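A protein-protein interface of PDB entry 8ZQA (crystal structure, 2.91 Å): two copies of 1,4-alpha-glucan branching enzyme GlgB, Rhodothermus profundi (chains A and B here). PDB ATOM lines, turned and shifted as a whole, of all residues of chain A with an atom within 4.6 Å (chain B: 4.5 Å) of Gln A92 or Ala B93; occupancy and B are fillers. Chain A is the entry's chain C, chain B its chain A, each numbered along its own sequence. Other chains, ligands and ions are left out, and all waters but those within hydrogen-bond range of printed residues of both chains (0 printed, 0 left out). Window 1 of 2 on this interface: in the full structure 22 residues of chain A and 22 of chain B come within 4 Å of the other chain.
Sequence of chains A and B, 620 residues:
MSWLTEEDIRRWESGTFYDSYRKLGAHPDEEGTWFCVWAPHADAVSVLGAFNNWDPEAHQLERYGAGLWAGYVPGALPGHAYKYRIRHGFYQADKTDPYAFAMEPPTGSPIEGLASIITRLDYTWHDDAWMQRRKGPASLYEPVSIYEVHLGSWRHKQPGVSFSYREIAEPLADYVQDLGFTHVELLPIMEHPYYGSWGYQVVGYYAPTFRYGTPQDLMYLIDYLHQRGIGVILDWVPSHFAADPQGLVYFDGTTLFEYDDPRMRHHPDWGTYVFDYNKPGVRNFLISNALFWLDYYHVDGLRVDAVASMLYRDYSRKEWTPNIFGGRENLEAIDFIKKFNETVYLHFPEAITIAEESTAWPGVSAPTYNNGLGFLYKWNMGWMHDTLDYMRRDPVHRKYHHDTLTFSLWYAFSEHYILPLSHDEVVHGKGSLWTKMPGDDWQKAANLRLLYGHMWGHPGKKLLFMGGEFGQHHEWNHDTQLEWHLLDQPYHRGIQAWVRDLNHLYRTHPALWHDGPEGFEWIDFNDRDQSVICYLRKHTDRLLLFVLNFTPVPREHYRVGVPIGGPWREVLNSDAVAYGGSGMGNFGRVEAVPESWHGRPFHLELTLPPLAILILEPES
Among the printed residues, pairs that only touch across the chains: Tyr A91 with Asp B94 (3.5 Å), Gln A92 with Ala B93 (3.6 Å), Tyr A91 with Lys B95 (3.6 Å), Ala A93 with Gln B92 (3.8 Å) and Gln A92 with Arg B85 (3.9 Å).
Arg A85 touches Gln B92, and with the chains exchanged Gln A92 touches Arg B85. Gln A92 touches Ala B93, and with the chains exchanged Ala A93 touches Gln B92. Positions printed for both chains: 85, 86, 92 and 93.
The side-chain amide oxygen of Gln B92 lies within hydrogen-bond range of the guanidinium group of Arg A85 (2.6 Å). The backbone NH of Asp B94 lies within hydrogen-bond range of the backbone carbonyl oxygen of Gln A92, at 2.7 Å.
Hydrophobic or aromatic side chains of chain A that line the printed part of chain B: Tyr A91. Along chain A the printed residues that touch a printed residue of chain B span positions 85 to 93. Among the printed residues, 7 pairs touch across the chains. Among the printed residues, no Asp or Glu carboxylate lies within 4 Å of a Lys or Arg side-chain nitrogen of the other chain.
The backbone carbonyl oxygen of Tyr B84 is in hydrogen-bond range of the backbone NH of Lys B95 (2.6 Å). NH1 of Arg B85 is in salt-bridge range of OD1 of Asp B94. O of Ile B86 is in hydrogen-bond range of N of Ala B93, at 2.9 Å. The backbone carbonyl oxygen (O) of Ile A86 sits at hydrogen-bond distance from the backbone NH (N) of Ala A93.
Arg A87 touches none of the printed residues of chain B. Gln A92 touches three residues of chain B. Of the printed residues of chain B, Ala A93 touches Gln B92. Printed residues of chain A within 4 Å of Arg B85: Gln A92. Ile B86 touches none of the printed residues of chain A. The nearest printed residue of chain A that does not touch Gln B92 is Gln A92 (4.8 Å).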
ATOM      1  N   ARG A  85      20.556   0.013 -14.021  1.00  0.00           N
ATOM      2  CA  ARG A  85      19.649   0.519 -12.996  1.00  0.00           C
ATOM      3  C   ARG A  85      19.473   2.003 -13.247  1.00  0.00           C
ATOM      4  O   ARG A  85      20.405   2.791 -13.026  1.00  0.00           O
ATOM      5  CB  ARG A  85      20.172   0.266 -11.583  1.00  0.00           C
ATOM      6  CG  ARG A  85      19.093   0.465 -10.530  1.00  0.00           C
ATOM      7  CD  ARG A  85      19.427  -0.213  -9.224  1.00  0.00           C
ATOM      8  NE  ARG A  85      18.907  -1.573  -9.191  1.00  0.00           N
ATOM      9  CZ  ARG A  85      18.811  -2.309  -8.093  1.00  0.00           C
ATOM     10  NH1 ARG A  85      19.195  -1.845  -6.915  1.00  0.00           N
ATOM     11  NH2 ARG A  85      18.329  -3.546  -8.182  1.00  0.00           N
ATOM     12  N   ILE A  86      18.301   2.387 -13.730  1.00  0.00           N
ATOM     13  CA  ILE A  86      18.015   3.775 -14.061  1.00  0.00           C
ATOM     14  C   ILE A  86      17.087   4.337 -13.005  1.00  0.00           C
ATOM     15  O   ILE A  86      16.064   3.719 -12.669  1.00  0.00           O
ATOM     16  CB  ILE A  86      17.407   3.888 -15.473  1.00  0.00           C
ATOM     17  CG1 ILE A  86      18.464   3.535 -16.512  1.00  0.00           C
ATOM     18  CG2 ILE A  86      16.918   5.298 -15.731  1.00  0.00           C
ATOM     19  CD1 ILE A  86      17.941   2.794 -17.712  1.00  0.00           C
ATOM     20  N   ARG A  87      17.417   5.513 -12.501  1.00  0.00           N
ATOM     21  CA  ARG A  87      16.653   6.169 -11.450  1.00  0.00           C
ATOM     22  C   ARG A  87      15.933   7.344 -12.082  1.00  0.00           C
ATOM     23  O   ARG A  87      16.575   8.259 -12.612  1.00  0.00           O
ATOM     24  CB  ARG A  87      17.553   6.620 -10.306  1.00  0.00           C
ATOM     25  CG  ARG A  87      16.885   6.545  -8.941  1.00  0.00           C
ATOM     26  CD  ARG A  87      17.529   7.511  -7.973  1.00  0.00           C
ATOM     27  NE  ARG A  87      17.074   8.880  -8.186  1.00  0.00           N
ATOM     28  CZ  ARG A  87      17.876   9.906  -8.436  1.00  0.00           C
ATOM     29  NH1 ARG A  87      19.192   9.769  -8.441  1.00  0.00           N
ATOM     30  NH2 ARG A  87      17.345  11.106  -8.645  1.00  0.00           N
ATOM     31  N   PHE A  90      12.021   9.773  -7.950  1.00  0.00           N
ATOM     32  CA  PHE A  90      11.675   8.949  -6.799  1.00  0.00           C
ATOM     33  C   PHE A  90      11.809   7.459  -7.094  1.00  0.00           C
ATOM     34  O   PHE A  90      12.053   6.670  -6.174  1.00  0.00           O
ATOM     35  CB  PHE A  90      10.252   9.272  -6.345  1.00  0.00           C
ATOM     36  CG  PHE A  90       9.949   8.829  -4.948  1.00  0.00           C
ATOM     37  CD1 PHE A  90      10.674   9.325  -3.881  1.00  0.00           C
ATOM     38  CD2 PHE A  90       8.930   7.925  -4.698  1.00  0.00           C
ATOM     39  CE1 PHE A  90      10.395   8.927  -2.595  1.00  0.00           C
ATOM     40  CE2 PHE A  90       8.645   7.520  -3.409  1.00  0.00           C
ATOM     41  CZ  PHE A  90       9.379   8.024  -2.355  1.00  0.00           C
ATOM     42  N   TYR A  91      11.654   7.051  -8.353  1.00  0.00           N
ATOM     43  CA  TYR A  91      11.541   5.643  -8.701  1.00  0.00           C
ATOM     44  C   TYR A  91      12.776   5.164  -9.453  1.00  0.00           C
ATOM     45  O   TYR A  91      13.388   5.905 -10.228  1.00  0.00           O
ATOM     46  CB  TYR A  91      10.274   5.398  -9.524  1.00  0.00           C
ATOM     47  CG  TYR A  91       9.034   5.580  -8.681  1.00  0.00           C
ATOM     48  CD1 TYR A  91       8.577   4.562  -7.854  1.00  0.00           C
ATOM     49  CD2 TYR A  91       8.358   6.792  -8.662  1.00  0.00           C
ATOM     50  CE1 TYR A  91       7.457   4.733  -7.064  1.00  0.00           C
ATOM     51  CE2 TYR A  91       7.237   6.971  -7.877  1.00  0.00           C
ATOM     52  CZ  TYR A  91       6.792   5.941  -7.079  1.00  0.00           C
ATOM     53  OH  TYR A  91       5.683   6.121  -6.288  1.00  0.00           O
ATOM     54  N   GLN A  92      13.117   3.900  -9.215  1.00  0.00           N
ATOM     55  CA  GLN A  92      14.240   3.227  -9.843  1.00  0.00           C
ATOM     56  C   GLN A  92      13.742   1.956 -10.516  1.00  0.00           C
ATOM     57  O   GLN A  92      12.781   1.330 -10.058  1.00  0.00           O
ATOM     58  CB  GLN A  92      15.289   2.887  -8.777  1.00  0.00           C
ATOM     59  CG  GLN A  92      16.736   2.923  -9.193  1.00  0.00           C
ATOM     60  CD  GLN A  92      17.635   3.237  -8.007  1.00  0.00           C
ATOM     61  OE1 GLN A  92      17.150   3.504  -6.905  1.00  0.00           O
ATOM     62  NE2 GLN A  92      18.943   3.187  -8.221  1.00  0.00           N
ATOM     63  N   ALA A  93      14.409   1.556 -11.593  1.00  0.00           N
ATOM     64  CA  ALA A  93      13.977   0.379 -12.333  1.00  0.00           C
ATOM     65  C   ALA A  93      15.178  -0.267 -13.006  1.00  0.00           C
ATOM     66  O   ALA A  93      16.106   0.419 -13.428  1.00  0.00           O
ATOM     67  CB  ALA A  93      12.910   0.734 -13.377  1.00  0.00           C
ATOM     68  N   TYR B  84       7.165   0.522  -3.147  1.00  0.00           N
ATOM     69  CA  TYR B  84       7.303  -0.921  -3.269  1.00  0.00           C
ATOM     70  C   TYR B  84       8.407  -1.244  -4.267  1.00  0.00           C
ATOM     71  O   TYR B  84       8.439  -0.684  -5.368  1.00  0.00           O
ATOM     72  CB  TYR B  84       5.977  -1.560  -3.683  1.00  0.00           C
ATOM     73  CG  TYR B  84       4.950  -1.530  -2.572  1.00  0.00           C
ATOM     74  CD1 TYR B  84       5.323  -1.770  -1.255  1.00  0.00           C
ATOM     75  CD2 TYR B  84       3.612  -1.257  -2.834  1.00  0.00           C
ATOM     76  CE1 TYR B  84       4.396  -1.739  -0.230  1.00  0.00           C
ATOM     77  CE2 TYR B  84       2.677  -1.225  -1.813  1.00  0.00           C
ATOM     78  CZ  TYR B  84       3.076  -1.463  -0.514  1.00  0.00           C
ATOM     79  OH  TYR B  84       2.148  -1.441   0.502  1.00  0.00           O
ATOM     80  N   ARG B  85       9.309  -2.139  -3.873  1.00  0.00           N
ATOM     81  CA  ARG B  85      10.367  -2.660  -4.735  1.00  0.00           C
ATOM     82  C   ARG B  85      10.031  -4.116  -5.028  1.00  0.00           C
ATOM     83  O   ARG B  85      10.142  -4.973  -4.145  1.00  0.00           O
ATOM     84  CB  ARG B  85      11.734  -2.519  -4.061  1.00  0.00           C
ATOM     85  CG  ARG B  85      12.932  -3.064  -4.848  1.00  0.00           C
ATOM     86  CD  ARG B  85      13.699  -1.985  -5.615  1.00  0.00           C
ATOM     87  NE  ARG B  85      14.920  -1.562  -4.937  1.00  0.00           N
ATOM     88  CZ  ARG B  85      15.390  -0.321  -4.942  1.00  0.00           C
ATOM     89  NH1 ARG B  85      14.776   0.649  -5.600  1.00  0.00           N
ATOM     90  NH2 ARG B  85      16.509  -0.047  -4.278  1.00  0.00           N
ATOM     91  N   ILE B  86       9.612  -4.394  -6.262  1.00  0.00           N
ATOM     92  CA  ILE B  86       9.186  -5.726  -6.680  1.00  0.00           C
ATOM     93  C   ILE B  86      10.269  -6.316  -7.569  1.00  0.00           C
ATOM     94  O   ILE B  86      10.802  -5.635  -8.452  1.00  0.00           O
ATOM     95  CB  ILE B  86       7.834  -5.691  -7.415  1.00  0.00           C
ATOM     96  CG1 ILE B  86       6.734  -5.201  -6.476  1.00  0.00           C
ATOM     97  CG2 ILE B  86       7.486  -7.067  -7.962  1.00  0.00           C
ATOM     98  CD1 ILE B  86       6.137  -3.882  -6.883  1.00  0.00           C
ATOM     99  N   GLN B  92      14.386  -5.894 -10.959  1.00  0.00           N
ATOM    100  CA  GLN B  92      13.523  -5.309  -9.936  1.00  0.00           C
ATOM    101  C   GLN B  92      13.176  -3.876 -10.321  1.00  0.00           C
ATOM    102  O   GLN B  92      13.910  -3.215 -11.058  1.00  0.00           O
ATOM    103  CB  GLN B  92      14.129  -5.324  -8.533  1.00  0.00           C
ATOM    104  CG  GLN B  92      15.032  -6.477  -8.221  1.00  0.00           C
ATOM    105  CD  GLN B  92      16.131  -6.057  -7.287  1.00  0.00           C
ATOM    106  OE1 GLN B  92      16.392  -4.866  -7.127  1.00  0.00           O
ATOM    107  NE2 GLN B  92      16.763  -7.024  -6.637  1.00  0.00           N
ATOM    108  N   ALA B  93      12.051  -3.392  -9.792  1.00  0.00           N
ATOM    109  CA  ALA B  93      11.545  -2.067 -10.125  1.00  0.00           C
ATOM    110  C   ALA B  93      10.816  -1.472  -8.929  1.00  0.00           C
ATOM    111  O   ALA B  93      10.307  -2.197  -8.068  1.00  0.00           O
ATOM    112  CB  ALA B  93      10.609  -2.108 -11.339  1.00  0.00           C
ATOM    113  N   ASP B  94      10.815  -0.142  -8.861  1.00  0.00           N
ATOM    114  CA  ASP B  94      10.080   0.596  -7.841  1.00  0.00           C
ATOM    115  C   ASP B  94       8.671   0.909  -8.334  1.00  0.00           C
ATOM    116  O   ASP B  94       8.494   1.371  -9.466  1.00  0.00           O
ATOM    117  CB  ASP B  94      10.808   1.896  -7.493  1.00  0.00           C
ATOM    118  CG  ASP B  94      11.989   1.679  -6.568  1.00  0.00           C
ATOM    119  OD1 ASP B  94      12.136   0.554  -6.056  1.00  0.00           O
ATOM    120  OD2 ASP B  94      12.767   2.632  -6.350  1.00  0.00           O
ATOM    121  N   LYS B  95       7.674   0.677  -7.478  1.00  0.00           N
ATOM    122  CA  LYS B  95       6.273   0.870  -7.828  1.00  0.00           C
ATOM    123  C   LYS B  95       5.552   1.669  -6.748  1.00  0.00           C
ATOM    124  O   LYS B  95       5.952   1.683  -5.582  1.00  0.00           O
ATOM    125  CB  LYS B  95       5.536  -0.465  -8.035  1.00  0.00           C
ATOM    126  CG  LYS B  95       5.886  -1.212  -9.307  1.00  0.00           C
ATOM    127  CD  LYS B  95       6.036  -0.276 -10.484  1.00  0.00           C
ATOM    128  CE  LYS B  95       5.569  -0.930 -11.771  1.00  0.00           C
ATOM    129  NZ  LYS B  95       4.657  -0.049 -12.555  1.00  0.00           N
